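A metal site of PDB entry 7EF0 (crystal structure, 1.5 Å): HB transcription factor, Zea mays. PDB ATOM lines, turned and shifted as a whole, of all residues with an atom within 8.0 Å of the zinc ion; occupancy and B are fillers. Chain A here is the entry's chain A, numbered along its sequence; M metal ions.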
ATOM      1  N   GLU A  71      18.566  -5.370  21.793  1.00  0.00           N
ATOM      2  CA  GLU A  71      17.587  -5.646  22.842  1.00  0.00           C
ATOM      3  C   GLU A  71      16.600  -6.690  22.400  1.00  0.00           C
ATOM      4  O   GLU A  71      16.395  -6.881  21.206  1.00  0.00           O
ATOM      5  CB  GLU A  71      16.870  -4.369  23.249  1.00  0.00           C
ATOM      6  CG  GLU A  71      17.733  -3.435  24.085  1.00  0.00           C
ATOM      7  CD  GLU A  71      17.062  -2.125  24.390  1.00  0.00           C
ATOM      8  OE1 GLU A  71      15.843  -1.994  24.103  1.00  0.00           O
ATOM      9  OE2 GLU A  71      17.754  -1.226  24.921  1.00  0.00           O
ATOM     10  N   ALA A  72      16.045  -7.398  23.366  1.00  0.00           N
ATOM     11  CA  ALA A  72      14.909  -8.289  23.173  1.00  0.00           C
ATOM     12  C   ALA A  72      15.138  -9.296  22.042  1.00  0.00           C
ATOM     13  O   ALA A  72      16.126 -10.014  22.039  1.00  0.00           O
ATOM     14  CB  ALA A  72      13.648  -7.462  22.927  1.00  0.00           C
ATOM     15  N   THR A  73      14.250  -9.346  21.060  1.00  0.00           N
ATOM     16  CA  THR A  73      14.381 -10.419  20.072  1.00  0.00           C
ATOM     17  C   THR A  73      15.248 -10.025  18.887  1.00  0.00           C
ATOM     18  O   THR A  73      15.382 -10.790  17.915  1.00  0.00           O
ATOM     19  CB  THR A  73      13.019 -10.885  19.565  1.00  0.00           C
ATOM     20  OG1 THR A  73      12.347  -9.775  18.956  1.00  0.00           O
ATOM     21  CG2 THR A  73      12.185 -11.434  20.720  1.00  0.00           C
ATOM     22  N   GLU A  74      15.891  -8.874  18.986  1.00  0.00           N
ATOM     23  CA  GLU A  74      16.905  -8.539  18.001  1.00  0.00           C
ATOM     24  C   GLU A  74      18.053  -9.559  18.049  1.00  0.00           C
ATOM     25  O   GLU A  74      18.878  -9.619  17.133  1.00  0.00           O
ATOM     26  CB  GLU A  74      17.437  -7.102  18.221  1.00  0.00           C
ATOM     27  CG  GLU A  74      16.371  -6.036  17.962  1.00  0.00           C
ATOM     28  CD  GLU A  74      16.602  -4.755  18.763  1.00  0.00           C
ATOM     29  OE1 GLU A  74      17.735  -4.508  19.231  1.00  0.00           O
ATOM     30  OE2 GLU A  74      15.638  -3.975  18.916  1.00  0.00           O
ATOM     31  N   CYS A  75      18.113 -10.377  19.094  1.00  0.00           N
ATOM     32  CA  CYS A  75      19.126 -11.415  19.203  1.00  0.00           C
ATOM     33  C   CYS A  75      19.055 -12.384  18.031  1.00  0.00           C
ATOM     34  O   CYS A  75      20.050 -13.036  17.744  1.00  0.00           O
ATOM     35  CB  CYS A  75      18.971 -12.195  20.526  1.00  0.00           C
ATOM     36  SG  CYS A  75      17.400 -13.109  20.674  1.00  0.00           S
ATOM     37  N   VAL A  76      17.904 -12.474  17.338  1.00  0.00           N
ATOM     38  CA  VAL A  76      17.859 -13.402  16.205  1.00  0.00           C
ATOM     39  C   VAL A  76      18.774 -12.973  15.058  1.00  0.00           C
ATOM     40  O   VAL A  76      19.121 -13.785  14.182  1.00  0.00           O
ATOM     41  CB  VAL A  76      16.432 -13.601  15.650  1.00  0.00           C
ATOM     42  CG1 VAL A  76      15.508 -14.105  16.755  1.00  0.00           C
ATOM     43  CG2 VAL A  76      15.890 -12.333  14.997  1.00  0.00           C
ATOM     44  N   GLN A 105      24.017 -19.502  21.857  1.00  0.00           N
ATOM     45  CA  GLN A 105      23.235 -20.417  22.645  1.00  0.00           C
ATOM     46  C   GLN A 105      21.883 -19.795  22.920  1.00  0.00           C
ATOM     47  O   GLN A 105      21.794 -18.866  23.733  1.00  0.00           O
ATOM     48  CB  GLN A 105      23.952 -20.744  23.953  1.00  0.00           C
ATOM     49  CG  GLN A 105      23.248 -21.803  24.771  1.00  0.00           C
ATOM     50  CD  GLN A 105      23.965 -22.100  26.070  1.00  0.00           C
ATOM     51  OE1 GLN A 105      24.165 -21.196  26.890  1.00  0.00           O
ATOM     52  NE2 GLN A 105      24.371 -23.348  26.259  1.00  0.00           N
ATOM     53  N   ARG A 106      20.861 -20.283  22.229  1.00  0.00           N
ATOM     54  CA  ARG A 106      19.524 -19.705  22.367  1.00  0.00           C
ATOM     55  C   ARG A 106      18.904 -20.166  23.665  1.00  0.00           C
ATOM     56  O   ARG A 106      18.988 -21.344  24.030  1.00  0.00           O
ATOM     57  CB  ARG A 106      18.649 -20.103  21.182  1.00  0.00           C
ATOM     58  CG  ARG A 106      19.231 -19.717  19.836  1.00  0.00           C
ATOM     59  CD  ARG A 106      19.349 -18.213  19.733  1.00  0.00           C
ATOM     60  NE  ARG A 106      19.957 -17.797  18.465  1.00  0.00           N
ATOM     61  CZ  ARG A 106      20.321 -16.555  18.192  1.00  0.00           C
ATOM     62  NH1 ARG A 106      20.145 -15.587  19.083  1.00  0.00           N
ATOM     63  NH2 ARG A 106      20.871 -16.271  17.023  1.00  0.00           N
ATOM     64  N   ARG A 107      18.292 -19.234  24.386  1.00  0.00           N
ATOM     65  CA  ARG A 107      17.649 -19.546  25.661  1.00  0.00           C
ATOM     66  C   ARG A 107      16.306 -18.844  25.752  1.00  0.00           C
ATOM     67  O   ARG A 107      16.088 -17.823  25.099  1.00  0.00           O
ATOM     68  CB  ARG A 107      18.559 -19.134  26.837  1.00  0.00           C
ATOM     69  CG  ARG A 107      19.854 -19.954  26.904  1.00  0.00           C
ATOM     70  CD  ARG A 107      20.851 -19.344  27.883  1.00  0.00           C
ATOM     71  NE  ARG A 107      20.691 -19.845  29.235  1.00  0.00           N
ATOM     72  CZ  ARG A 107      20.738 -19.092  30.336  1.00  0.00           C
ATOM     73  NH1 ARG A 107      20.932 -17.782  30.258  1.00  0.00           N
ATOM     74  NH2 ARG A 107      20.585 -19.662  31.532  1.00  0.00           N
ATOM     75  N   ARG A 108      15.438 -19.390  26.570  1.00  0.00           N
ATOM     76  CA  ARG A 108      14.116 -18.829  26.851  1.00  0.00           C
ATOM     77  C   ARG A 108      14.210 -17.356  27.255  1.00  0.00           C
ATOM     78  O   ARG A 108      14.942 -17.020  28.178  1.00  0.00           O
ATOM     79  CB  ARG A 108      13.459 -19.674  27.943  1.00  0.00           C
ATOM     80  CG  ARG A 108      12.089 -19.244  28.439  1.00  0.00           C
ATOM     81  CD  ARG A 108      11.715 -20.018  29.736  1.00  0.00           C
ATOM     82  NE  ARG A 108      12.809 -20.034  30.710  1.00  0.00           N
ATOM     83  CZ  ARG A 108      13.116 -19.026  31.522  1.00  0.00           C
ATOM     84  NH1 ARG A 108      12.394 -17.912  31.527  1.00  0.00           N
ATOM     85  NH2 ARG A 108      14.148 -19.122  32.349  1.00  0.00           N
ATOM     86  N   HIS A 109      13.477 -16.488  26.567  1.00  0.00           N
ATOM     87  CA  HIS A 109      13.377 -15.089  27.020  1.00  0.00           C
ATOM     88  C   HIS A 109      12.409 -14.929  28.192  1.00  0.00           C
ATOM     89  O   HIS A 109      11.575 -15.798  28.451  1.00  0.00           O
ATOM     90  CB  HIS A 109      12.942 -14.183  25.851  1.00  0.00           C
ATOM     91  CG  HIS A 109      14.012 -13.958  24.839  1.00  0.00           C
ATOM     92  ND1 HIS A 109      14.051 -12.836  24.042  1.00  0.00           N
ATOM     93  CD2 HIS A 109      15.121 -14.684  24.525  1.00  0.00           C
ATOM     94  CE1 HIS A 109      15.117 -12.888  23.262  1.00  0.00           C
ATOM     95  NE2 HIS A 109      15.779 -14.001  23.518  1.00  0.00           N
ATOM     96  N   GLY A 113      13.731  -9.723  28.896  1.00  0.00           N
ATOM     97  CA  GLY A 113      14.165  -9.852  27.523  1.00  0.00           C
ATOM     98  C   GLY A 113      15.029 -11.066  27.263  1.00  0.00           C
ATOM     99  O   GLY A 113      14.750 -12.170  27.711  1.00  0.00           O
ATOM    100  N   CYS A 114      16.101 -10.850  26.511  1.00  0.00           N
ATOM    101  CA  CYS A 114      16.925 -11.925  25.984  1.00  0.00           C
ATOM    102  C   CYS A 114      17.796 -12.579  27.051  1.00  0.00           C
ATOM    103  O   CYS A 114      18.453 -11.889  27.818  1.00  0.00           O
ATOM    104  CB  CYS A 114      17.788 -11.380  24.852  1.00  0.00           C
ATOM    105  SG  CYS A 114      18.945 -12.562  24.122  1.00  0.00           S
ATOM    106  N   ARG A 115      17.814 -13.914  27.066  1.00  0.00           N
ATOM    107  CA  ARG A 115      18.710 -14.696  27.914  1.00  0.00           C
ATOM    108  C   ARG A 115      19.743 -15.489  27.106  1.00  0.00           C
ATOM    109  O   ARG A 115      20.511 -16.275  27.663  1.00  0.00           O
ATOM    110  CB  ARG A 115      17.903 -15.671  28.790  1.00  0.00           C
ATOM    111  CG  ARG A 115      17.251 -14.988  29.959  1.00  0.00           C
ATOM    112  CD  ARG A 115      16.335 -15.924  30.744  1.00  0.00           C
ATOM    113  NE  ARG A 115      17.048 -16.954  31.488  1.00  0.00           N
ATOM    114  CZ  ARG A 115      17.096 -18.244  31.136  1.00  0.00           C
ATOM    115  NH1 ARG A 115      16.516 -18.665  30.016  1.00  0.00           N
ATOM    116  NH2 ARG A 115      17.760 -19.106  31.900  1.00  0.00           N
ATOM    117  N   CYS A 116      19.774 -15.265  25.798  1.00  0.00           N
ATOM    118  CA  CYS A 116      20.726 -15.966  24.956  1.00  0.00           C
ATOM    119  C   CYS A 116      22.163 -15.637  25.349  1.00  0.00           C
ATOM    120  O   CYS A 116      22.448 -14.571  25.894  1.00  0.00           O
ATOM    121  CB  CYS A 116      20.502 -15.603  23.484  1.00  0.00           C
ATOM    122  SG  CYS A 116      18.837 -16.038  22.866  1.00  0.00           S
ATOM    123  N   ARG A 117      23.056 -16.587  25.099  1.00  0.00           N
ATOM    124  CA  ARG A 117      24.469 -16.394  25.433  1.00  0.00           C
ATOM    125  C   ARG A 117      25.333 -16.572  24.211  1.00  0.00           C
ATOM    126  O   ARG A 117      25.139 -17.502  23.424  1.00  0.00           O
ATOM    127  CB  ARG A 117      24.884 -17.356  26.539  1.00  0.00           C
ATOM    128  CG  ARG A 117      24.176 -17.113  27.849  1.00  0.00           C
ATOM    129  CD  ARG A 117      24.690 -18.035  28.942  1.00  0.00           C
ATOM    130  NE  ARG A 117      24.117 -17.719  30.242  1.00  0.00           N
ATOM    131  CZ  ARG A 117      24.685 -18.014  31.406  1.00  0.00           C
ATOM    132  NH1 ARG A 117      25.851 -18.630  31.426  1.00  0.00           N
ATOM    133  NH2 ARG A 117      24.086 -17.690  32.533  1.00  0.00           N
ATOM    134  N   PHE A 118      26.306 -15.686  24.066  1.00  0.00           N
ATOM    135  CA  PHE A 118      27.134 -15.692  22.864  1.00  0.00           C
ATOM    136  C   PHE A 118      28.586 -15.917  23.203  1.00  0.00           C
ATOM    137  O   PHE A 118      29.174 -15.155  23.958  1.00  0.00           O
ATOM    138  CB  PHE A 118      26.970 -14.376  22.109  1.00  0.00           C
ATOM    139  CG  PHE A 118      25.538 -14.084  21.776  1.00  0.00           C
ATOM    140  CD1 PHE A 118      25.001 -14.557  20.594  1.00  0.00           C
ATOM    141  CD2 PHE A 118      24.732 -13.392  22.665  1.00  0.00           C
ATOM    142  CE1 PHE A 118      23.671 -14.327  20.296  1.00  0.00           C
ATOM    143  CE2 PHE A 118      23.403 -13.170  22.373  1.00  0.00           C
ATOM    144  CZ  PHE A 118      22.873 -13.637  21.180  1.00  0.00           C
ATOM    145  N   LEU A 133      23.375 -10.461  25.829  1.00  0.00           N
ATOM    146  CA  LEU A 133      23.042  -9.513  24.786  1.00  0.00           C
ATOM    147  C   LEU A 133      23.378  -8.068  25.133  1.00  0.00           C
ATOM    148  O   LEU A 133      23.652  -7.263  24.236  1.00  0.00           O
ATOM    149  CB  LEU A 133      21.544  -9.629  24.435  1.00  0.00           C
ATOM    150  CG  LEU A 133      21.166  -8.990  23.099  1.00  0.00           C
ATOM    151  CD1 LEU A 133      21.762  -9.798  21.943  1.00  0.00           C
ATOM    152  CD2 LEU A 133      19.681  -8.892  22.957  1.00  0.00           C
ATOM    153  N   ALA A 152      11.070 -16.544  14.284  1.00  0.00           N
ATOM    154  CA  ALA A 152      12.011 -16.835  15.372  1.00  0.00           C
ATOM    155  C   ALA A 152      11.874 -15.785  16.479  1.00  0.00           C
ATOM    156  O   ALA A 152      12.043 -16.092  17.654  1.00  0.00           O
ATOM    157  CB  ALA A 152      13.433 -16.887  14.851  1.00  0.00           C
ATOM    158  N   ALA A 156      10.696 -16.635  20.420  1.00  0.00           N
ATOM    159  CA  ALA A 156      11.474 -16.192  21.579  1.00  0.00           C
ATOM    160  C   ALA A 156      10.629 -15.418  22.579  1.00  0.00           C
ATOM    161  O   ALA A 156      10.719 -15.645  23.778  1.00  0.00           O
ATOM    162  CB  ALA A 156      12.656 -15.347  21.131  1.00  0.00           C
HETATM  163 ZN    ZN M   1      17.728 -14.001  22.787  1.00  0.00          ZN
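The side-chain sulfur (SG) of Cys 75 lies close to the backbone carbonyl oxygen (O) of Ala 72 (3.6 Å). O of Cys 75 sits at hydrogen-bond distance from NH1 of Arg 106, 2.9 Å away. SG of Cys 116 sits close to N of Arg 107, 3.6 Å away.
Of the 20 residues printed, 4 come within 4 Å of the zinc ion.
The zinc ion is bound by NE2 of His 109, SG of Cys 114, SG of Cys 75 and SG of Cys 116.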
